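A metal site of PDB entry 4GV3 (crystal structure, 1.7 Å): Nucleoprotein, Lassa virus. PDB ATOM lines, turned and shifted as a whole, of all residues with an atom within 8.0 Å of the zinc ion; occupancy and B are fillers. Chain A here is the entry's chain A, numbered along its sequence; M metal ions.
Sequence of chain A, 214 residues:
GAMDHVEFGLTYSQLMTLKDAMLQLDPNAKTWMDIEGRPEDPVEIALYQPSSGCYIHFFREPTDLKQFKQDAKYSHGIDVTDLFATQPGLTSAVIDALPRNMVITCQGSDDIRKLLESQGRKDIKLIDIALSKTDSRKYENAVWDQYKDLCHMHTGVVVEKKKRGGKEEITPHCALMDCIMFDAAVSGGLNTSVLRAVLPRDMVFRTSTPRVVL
The side-chain carboxylate (OE2) of Glu 44 lies close to a ring nitrogen (NE2) of His 57 (2.7 Å). OE1 of Glu 44 lies within hydrogen-bond range of N of Ala 175, 3.0 Å away. The backbone carbonyl oxygen of Glu 44 is in hydrogen-bond range of the backbone NH of Glu 36. A ring nitrogen (ND1) of His 154 sits close to the backbone carbonyl oxygen (O) of His 173, 3.3 Å away. A ring nitrogen (ND1) of His 154 sits at hydrogen-bond distance from the backbone carbonyl oxygen of His 76 (2.6 Å). The side-chain sulfur (SG) of Cys 174 lies close to the backbone NH (N) of Leu 176. SG of Cys 174 lies close to N of Met 177 (3.5 Å).
Residues that only touch the zinc ion: His 57 (3.8 Å). Five residues have an atom within 4 Å of the zinc ion: Glu 44, His 57, Cys 151, His 154 and Cys 174.
The zinc ion is bound by OE2 of Glu 44 (2.1 Å). NE2 of His 154 is bound to the zinc ion, at 2.1 Å. SG of Cys 174 is bound to the zinc ion, 2.3 Å away. The zinc ion is bound by SG of Cys 151.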
ATOM      1  N   GLU A  36     -27.774 -16.940 -20.613  1.00  0.00           N
ATOM      2  CA  GLU A  36     -28.874 -16.907 -19.670  1.00  0.00           C
ATOM      3  C   GLU A  36     -29.916 -15.957 -20.222  1.00  0.00           C
ATOM      4  O   GLU A  36     -29.587 -15.018 -20.938  1.00  0.00           O
ATOM      5  CB  GLU A  36     -28.418 -16.502 -18.263  1.00  0.00           C
ATOM      6  CG  GLU A  36     -27.314 -17.372 -17.675  1.00  0.00           C
ATOM      7  CD  GLU A  36     -27.635 -18.856 -17.624  1.00  0.00           C
ATOM      8  OE1 GLU A  36     -28.822 -19.224 -17.454  1.00  0.00           O
ATOM      9  OE2 GLU A  36     -26.700 -19.672 -17.736  1.00  0.00           O
ATOM     10  N   GLU A  44     -27.505 -12.610 -20.570  1.00  0.00           N
ATOM     11  CA  GLU A  44     -26.088 -12.881 -20.375  1.00  0.00           C
ATOM     12  C   GLU A  44     -25.577 -13.818 -21.476  1.00  0.00           C
ATOM     13  O   GLU A  44     -26.203 -14.828 -21.773  1.00  0.00           O
ATOM     14  CB  GLU A  44     -25.841 -13.498 -19.004  1.00  0.00           C
ATOM     15  CG  GLU A  44     -24.367 -13.656 -18.674  1.00  0.00           C
ATOM     16  CD  GLU A  44     -24.105 -14.322 -17.340  1.00  0.00           C
ATOM     17  OE1 GLU A  44     -24.891 -15.210 -16.958  1.00  0.00           O
ATOM     18  OE2 GLU A  44     -23.115 -13.956 -16.691  1.00  0.00           O
ATOM     19  N   ILE A  45     -24.428 -13.455 -22.050  1.00  0.00           N
ATOM     20  CA  ILE A  45     -23.822 -14.257 -23.107  1.00  0.00           C
ATOM     21  C   ILE A  45     -22.369 -14.519 -22.758  1.00  0.00           C
ATOM     22  O   ILE A  45     -21.655 -13.631 -22.300  1.00  0.00           O
ATOM     23  CB  ILE A  45     -23.956 -13.588 -24.484  1.00  0.00           C
ATOM     24  CG1 ILE A  45     -25.438 -13.559 -24.904  1.00  0.00           C
ATOM     25  CG2 ILE A  45     -23.098 -14.308 -25.525  1.00  0.00           C
ATOM     26  CD1 ILE A  45     -25.738 -12.833 -26.183  1.00  0.00           C
ATOM     27  N   ALA A  46     -21.935 -15.761 -22.968  1.00  0.00           N
ATOM     28  CA  ALA A  46     -20.536 -16.120 -22.782  1.00  0.00           C
ATOM     29  C   ALA A  46     -20.073 -17.044 -23.904  1.00  0.00           C
ATOM     30  O   ALA A  46     -20.809 -17.921 -24.359  1.00  0.00           O
ATOM     31  CB  ALA A  46     -20.330 -16.781 -21.433  1.00  0.00           C
ATOM     32  N   HIS A  57     -17.666 -12.235 -22.526  1.00  0.00           N
ATOM     33  CA  HIS A  57     -18.700 -12.227 -21.503  1.00  0.00           C
ATOM     34  C   HIS A  57     -19.350 -10.865 -21.412  1.00  0.00           C
ATOM     35  O   HIS A  57     -18.679  -9.859 -21.188  1.00  0.00           O
ATOM     36  CB  HIS A  57     -18.096 -12.631 -20.156  1.00  0.00           C
ATOM     37  CG  HIS A  57     -19.100 -12.749 -19.048  1.00  0.00           C
ATOM     38  ND1 HIS A  57     -18.826 -12.362 -17.761  1.00  0.00           N
ATOM     39  CD2 HIS A  57     -20.373 -13.221 -19.044  1.00  0.00           C
ATOM     40  CE1 HIS A  57     -19.880 -12.585 -17.001  1.00  0.00           C
ATOM     41  NE2 HIS A  57     -20.829 -13.107 -17.756  1.00  0.00           N
ATOM     42  N   PHE A  58     -20.661 -10.824 -21.635  1.00  0.00           N
ATOM     43  CA  PHE A  58     -21.383  -9.562 -21.589  1.00  0.00           C
ATOM     44  C   PHE A  58     -22.859  -9.766 -21.299  1.00  0.00           C
ATOM     45  O   PHE A  58     -23.361 -10.891 -21.281  1.00  0.00           O
ATOM     46  CB  PHE A  58     -21.180  -8.761 -22.880  1.00  0.00           C
ATOM     47  CG  PHE A  58     -21.710  -9.439 -24.111  1.00  0.00           C
ATOM     48  CD1 PHE A  58     -20.940 -10.345 -24.813  1.00  0.00           C
ATOM     49  CD2 PHE A  58     -22.983  -9.154 -24.576  1.00  0.00           C
ATOM     50  CE1 PHE A  58     -21.427 -10.973 -25.943  1.00  0.00           C
ATOM     51  CE2 PHE A  58     -23.478  -9.771 -25.707  1.00  0.00           C
ATOM     52  CZ  PHE A  58     -22.694 -10.681 -26.394  1.00  0.00           C
ATOM     53  N   PHE A  59     -23.552  -8.651 -21.067  1.00  0.00           N
ATOM     54  CA  PHE A  59     -24.916  -8.673 -20.585  1.00  0.00           C
ATOM     55  C   PHE A  59     -25.796  -7.822 -21.476  1.00  0.00           C
ATOM     56  O   PHE A  59     -25.327  -7.066 -22.319  1.00  0.00           O
ATOM     57  CB  PHE A  59     -24.958  -8.189 -19.134  1.00  0.00           C
ATOM     58  CG  PHE A  59     -23.931  -8.854 -18.255  1.00  0.00           C
ATOM     59  CD1 PHE A  59     -22.653  -8.331 -18.141  1.00  0.00           C
ATOM     60  CD2 PHE A  59     -24.246 -10.003 -17.565  1.00  0.00           C
ATOM     61  CE1 PHE A  59     -21.703  -8.941 -17.332  1.00  0.00           C
ATOM     62  CE2 PHE A  59     -23.300 -10.625 -16.763  1.00  0.00           C
ATOM     63  CZ  PHE A  59     -22.026 -10.097 -16.642  1.00  0.00           C
ATOM     64  N   HIS A  76     -31.197 -18.086 -13.255  1.00  0.00           N
ATOM     65  CA  HIS A  76     -29.995 -17.248 -13.286  1.00  0.00           C
ATOM     66  C   HIS A  76     -29.772 -16.325 -12.080  1.00  0.00           C
ATOM     67  O   HIS A  76     -28.642 -15.915 -11.831  1.00  0.00           O
ATOM     68  CB  HIS A  76     -29.863 -16.482 -14.619  1.00  0.00           C
ATOM     69  CG  HIS A  76     -31.039 -15.634 -14.986  1.00  0.00           C
ATOM     70  ND1 HIS A  76     -31.450 -14.557 -14.234  1.00  0.00           N
ATOM     71  CD2 HIS A  76     -31.866 -15.660 -16.063  1.00  0.00           C
ATOM     72  CE1 HIS A  76     -32.485 -13.968 -14.815  1.00  0.00           C
ATOM     73  NE2 HIS A  76     -32.749 -14.619 -15.932  1.00  0.00           N
ATOM     74  N   ILE A  78     -30.192 -13.268 -11.588  1.00  0.00           N
ATOM     75  CA  ILE A  78     -29.544 -12.014 -11.955  1.00  0.00           C
ATOM     76  C   ILE A  78     -30.392 -10.850 -11.459  1.00  0.00           C
ATOM     77  O   ILE A  78     -31.600 -10.809 -11.678  1.00  0.00           O
ATOM     78  CB  ILE A  78     -29.307 -11.884 -13.472  1.00  0.00           C
ATOM     79  CG1 ILE A  78     -28.332 -12.966 -13.960  1.00  0.00           C
ATOM     80  CG2 ILE A  78     -28.736 -10.502 -13.801  1.00  0.00           C
ATOM     81  CD1 ILE A  78     -28.267 -13.087 -15.471  1.00  0.00           C
ATOM     82  N   TRP A 144     -16.894 -22.466  -9.539  1.00  0.00           N
ATOM     83  CA  TRP A 144     -17.240 -21.279  -8.759  1.00  0.00           C
ATOM     84  C   TRP A 144     -16.143 -20.961  -7.744  1.00  0.00           C
ATOM     85  O   TRP A 144     -15.823 -19.786  -7.522  1.00  0.00           O
ATOM     86  CB  TRP A 144     -18.591 -21.428  -8.059  1.00  0.00           C
ATOM     87  CG  TRP A 144     -19.802 -21.177  -8.929  1.00  0.00           C
ATOM     88  CD1 TRP A 144     -20.618 -22.124  -9.480  1.00  0.00           C
ATOM     89  CD2 TRP A 144     -20.348 -19.913  -9.326  1.00  0.00           C
ATOM     90  NE1 TRP A 144     -21.626 -21.527 -10.195  1.00  0.00           N
ATOM     91  CE2 TRP A 144     -21.490 -20.174 -10.108  1.00  0.00           C
ATOM     92  CE3 TRP A 144     -19.977 -18.578  -9.089  1.00  0.00           C
ATOM     93  CZ2 TRP A 144     -22.268 -19.154 -10.670  1.00  0.00           C
ATOM     94  CZ3 TRP A 144     -20.751 -17.563  -9.644  1.00  0.00           C
ATOM     95  CH2 TRP A 144     -21.883 -17.852 -10.422  1.00  0.00           C
ATOM     96  N   LYS A 148     -15.267 -17.368  -9.263  1.00  0.00           N
ATOM     97  CA  LYS A 148     -16.341 -16.499  -8.763  1.00  0.00           C
ATOM     98  C   LYS A 148     -16.125 -14.997  -9.034  1.00  0.00           C
ATOM     99  O   LYS A 148     -17.094 -14.288  -9.303  1.00  0.00           O
ATOM    100  CB  LYS A 148     -16.598 -16.731  -7.277  1.00  0.00           C
ATOM    101  CG  LYS A 148     -15.357 -16.667  -6.399  1.00  0.00           C
ATOM    102  CD  LYS A 148     -15.724 -16.789  -4.933  1.00  0.00           C
ATOM    103  CE  LYS A 148     -14.485 -16.835  -4.061  1.00  0.00           C
ATOM    104  NZ  LYS A 148     -13.904 -18.203  -3.959  1.00  0.00           N
ATOM    105  N   LEU A 150     -15.126 -13.521 -11.519  1.00  0.00           N
ATOM    106  CA  LEU A 150     -15.372 -13.161 -12.914  1.00  0.00           C
ATOM    107  C   LEU A 150     -16.833 -12.796 -13.207  1.00  0.00           C
ATOM    108  O   LEU A 150     -17.118 -12.249 -14.264  1.00  0.00           O
ATOM    109  CB  LEU A 150     -14.918 -14.280 -13.851  1.00  0.00           C
ATOM    110  CG  LEU A 150     -13.435 -14.653 -13.827  1.00  0.00           C
ATOM    111  CD1 LEU A 150     -13.106 -15.721 -14.853  1.00  0.00           C
ATOM    112  CD2 LEU A 150     -12.561 -13.422 -14.031  1.00  0.00           C
ATOM    113  N   CYS A 151     -17.739 -13.073 -12.269  1.00  0.00           N
ATOM    114  CA  CYS A 151     -19.140 -12.648 -12.424  1.00  0.00           C
ATOM    115  C   CYS A 151     -19.863 -12.474 -11.092  1.00  0.00           C
ATOM    116  O   CYS A 151     -19.956 -13.412 -10.292  1.00  0.00           O
ATOM    117  CB  CYS A 151     -19.914 -13.624 -13.304  1.00  0.00           C
ATOM    118  SG  CYS A 151     -21.474 -12.907 -13.848  1.00  0.00           S
ATOM    119  N   HIS A 152     -20.407 -11.272 -10.885  1.00  0.00           N
ATOM    120  CA  HIS A 152     -21.048 -10.890  -9.623  1.00  0.00           C
ATOM    121  C   HIS A 152     -22.558 -10.667  -9.768  1.00  0.00           C
ATOM    122  O   HIS A 152     -23.206 -10.223  -8.818  1.00  0.00           O
ATOM    123  CB  HIS A 152     -20.387  -9.617  -9.099  1.00  0.00           C
ATOM    124  CG  HIS A 152     -18.913  -9.754  -8.857  1.00  0.00           C
ATOM    125  ND1 HIS A 152     -18.402 -10.114  -7.631  1.00  0.00           N
ATOM    126  CD2 HIS A 152     -17.848  -9.605  -9.681  1.00  0.00           C
ATOM    127  CE1 HIS A 152     -17.078 -10.167  -7.712  1.00  0.00           C
ATOM    128  NE2 HIS A 152     -16.725  -9.864  -8.942  1.00  0.00           N
ATOM    129  N   MET A 153     -23.103 -10.993 -10.934  1.00  0.00           N
ATOM    130  CA  MET A 153     -24.500 -10.691 -11.257  1.00  0.00           C
ATOM    131  C   MET A 153     -25.527 -11.586 -10.581  1.00  0.00           C
ATOM    132  O   MET A 153     -26.683 -11.198 -10.477  1.00  0.00           O
ATOM    133  CB  MET A 153     -24.726 -10.815 -12.765  1.00  0.00           C
ATOM    134  CG  MET A 153     -24.049  -9.727 -13.581  1.00  0.00           C
ATOM    135  SD  MET A 153     -24.851  -8.130 -13.425  1.00  0.00           S
ATOM    136  CE  MET A 153     -23.857  -7.176 -14.581  1.00  0.00           C
ATOM    137  N   HIS A 154     -25.097 -12.757 -10.111  1.00  0.00           N
ATOM    138  CA  HIS A 154     -26.027 -13.806  -9.676  1.00  0.00           C
ATOM    139  C   HIS A 154     -26.231 -13.848  -8.169  1.00  0.00           C
ATOM    140  O   HIS A 154     -25.808 -14.783  -7.496  1.00  0.00           O
ATOM    141  CB  HIS A 154     -25.525 -15.144 -10.192  1.00  0.00           C
ATOM    142  CG  HIS A 154     -25.224 -15.146 -11.656  1.00  0.00           C
ATOM    143  ND1 HIS A 154     -26.191 -15.423 -12.602  1.00  0.00           N
ATOM    144  CD2 HIS A 154     -24.101 -14.839 -12.343  1.00  0.00           C
ATOM    145  CE1 HIS A 154     -25.653 -15.324 -13.804  1.00  0.00           C
ATOM    146  NE2 HIS A 154     -24.388 -14.963 -13.672  1.00  0.00           N
ATOM    147  N   PRO A 172     -26.963 -20.473  -8.510  1.00  0.00           N
ATOM    148  CA  PRO A 172     -27.443 -19.845  -9.745  1.00  0.00           C
ATOM    149  C   PRO A 172     -26.666 -20.237 -10.998  1.00  0.00           C
ATOM    150  O   PRO A 172     -25.488 -20.585 -10.910  1.00  0.00           O
ATOM    151  CB  PRO A 172     -27.251 -18.349  -9.490  1.00  0.00           C
ATOM    152  CG  PRO A 172     -27.224 -18.197  -8.014  1.00  0.00           C
ATOM    153  CD  PRO A 172     -26.695 -19.484  -7.446  1.00  0.00           C
ATOM    154  N   HIS A 173     -27.331 -20.156 -12.143  1.00  0.00           N
ATOM    155  CA  HIS A 173     -26.719 -20.483 -13.434  1.00  0.00           C
ATOM    156  C   HIS A 173     -26.121 -19.228 -14.057  1.00  0.00           C
ATOM    157  O   HIS A 173     -26.814 -18.227 -14.252  1.00  0.00           O
ATOM    158  CB  HIS A 173     -27.750 -21.098 -14.362  1.00  0.00           C
ATOM    159  CG  HIS A 173     -28.163 -22.490 -13.972  1.00  0.00           C
ATOM    160  ND1 HIS A 173     -28.841 -23.332 -14.822  1.00  0.00           N
ATOM    161  CD2 HIS A 173     -27.974 -23.179 -12.823  1.00  0.00           C
ATOM    162  CE1 HIS A 173     -29.060 -24.483 -14.214  1.00  0.00           C
ATOM    163  NE2 HIS A 173     -28.546 -24.427 -13.003  1.00  0.00           N
ATOM    164  N   CYS A 174     -24.825 -19.294 -14.361  1.00  0.00           N
ATOM    165  CA  CYS A 174     -24.060 -18.217 -14.995  1.00  0.00           C
ATOM    166  C   CYS A 174     -23.566 -18.729 -16.350  1.00  0.00           C
ATOM    167  O   CYS A 174     -23.022 -19.828 -16.429  1.00  0.00           O
ATOM    168  CB  CYS A 174     -22.859 -17.842 -14.130  1.00  0.00           C
ATOM    169  SG  CYS A 174     -21.642 -16.713 -14.895  1.00  0.00           S
ATOM    170  N   ALA A 175     -23.762 -17.940 -17.408  1.00  0.00           N
ATOM    171  CA  ALA A 175     -23.333 -18.338 -18.750  1.00  0.00           C
ATOM    172  C   ALA A 175     -21.830 -18.635 -18.800  1.00  0.00           C
ATOM    173  O   ALA A 175     -21.405 -19.593 -19.445  1.00  0.00           O
ATOM    174  CB  ALA A 175     -23.686 -17.258 -19.768  1.00  0.00           C
ATOM    175  N   LEU A 176     -21.037 -17.814 -18.127  1.00  0.00           N
ATOM    176  CA  LEU A 176     -19.592 -18.010 -18.113  1.00  0.00           C
ATOM    177  C   LEU A 176     -19.182 -19.230 -17.285  1.00  0.00           C
ATOM    178  O   LEU A 176     -18.453 -20.098 -17.781  1.00  0.00           O
ATOM    179  CB  LEU A 176     -18.874 -16.760 -17.616  1.00  0.00           C
ATOM    180  CG  LEU A 176     -17.345 -16.799 -17.653  1.00  0.00           C
ATOM    181  CD1 LEU A 176     -16.821 -17.121 -19.040  1.00  0.00           C
ATOM    182  CD2 LEU A 176     -16.815 -15.455 -17.178  1.00  0.00           C
ATOM    183  N   MET A 177     -19.641 -19.317 -16.046  1.00  0.00           N
ATOM    184  CA  MET A 177     -19.316 -20.494 -15.217  1.00  0.00           C
ATOM    185  C   MET A 177     -19.806 -21.777 -15.900  1.00  0.00           C
ATOM    186  O   MET A 177     -19.126 -22.801 -15.840  1.00  0.00           O
ATOM    187  CB  MET A 177     -19.896 -20.394 -13.806  1.00  0.00           C
ATOM    188  CG  MET A 177     -19.511 -19.145 -13.047  1.00  0.00           C
ATOM    189  SD  MET A 177     -17.730 -18.903 -12.905  1.00  0.00           S
ATOM    190  CE  MET A 177     -17.674 -17.115 -12.987  1.00  0.00           C
ATOM    191  N   ASP A 178     -20.966 -21.721 -16.535  1.00  0.00           N
ATOM    192  CA  ASP A 178     -21.488 -22.877 -17.288  1.00  0.00           C
ATOM    193  C   ASP A 178     -20.486 -23.359 -18.344  1.00  0.00           C
ATOM    194  O   ASP A 178     -20.160 -24.540 -18.378  1.00  0.00           O
ATOM    195  CB  ASP A 178     -22.831 -22.554 -17.963  1.00  0.00           C
ATOM    196  CG  ASP A 178     -24.029 -22.736 -17.037  1.00  0.00           C
ATOM    197  OD1 ASP A 178     -23.837 -23.015 -15.832  1.00  0.00           O
ATOM    198  OD2 ASP A 178     -25.176 -22.608 -17.520  1.00  0.00           O
HETATM  199 ZN    ZN M   1     -22.642 -14.671 -14.786  1.00  0.00          ZN
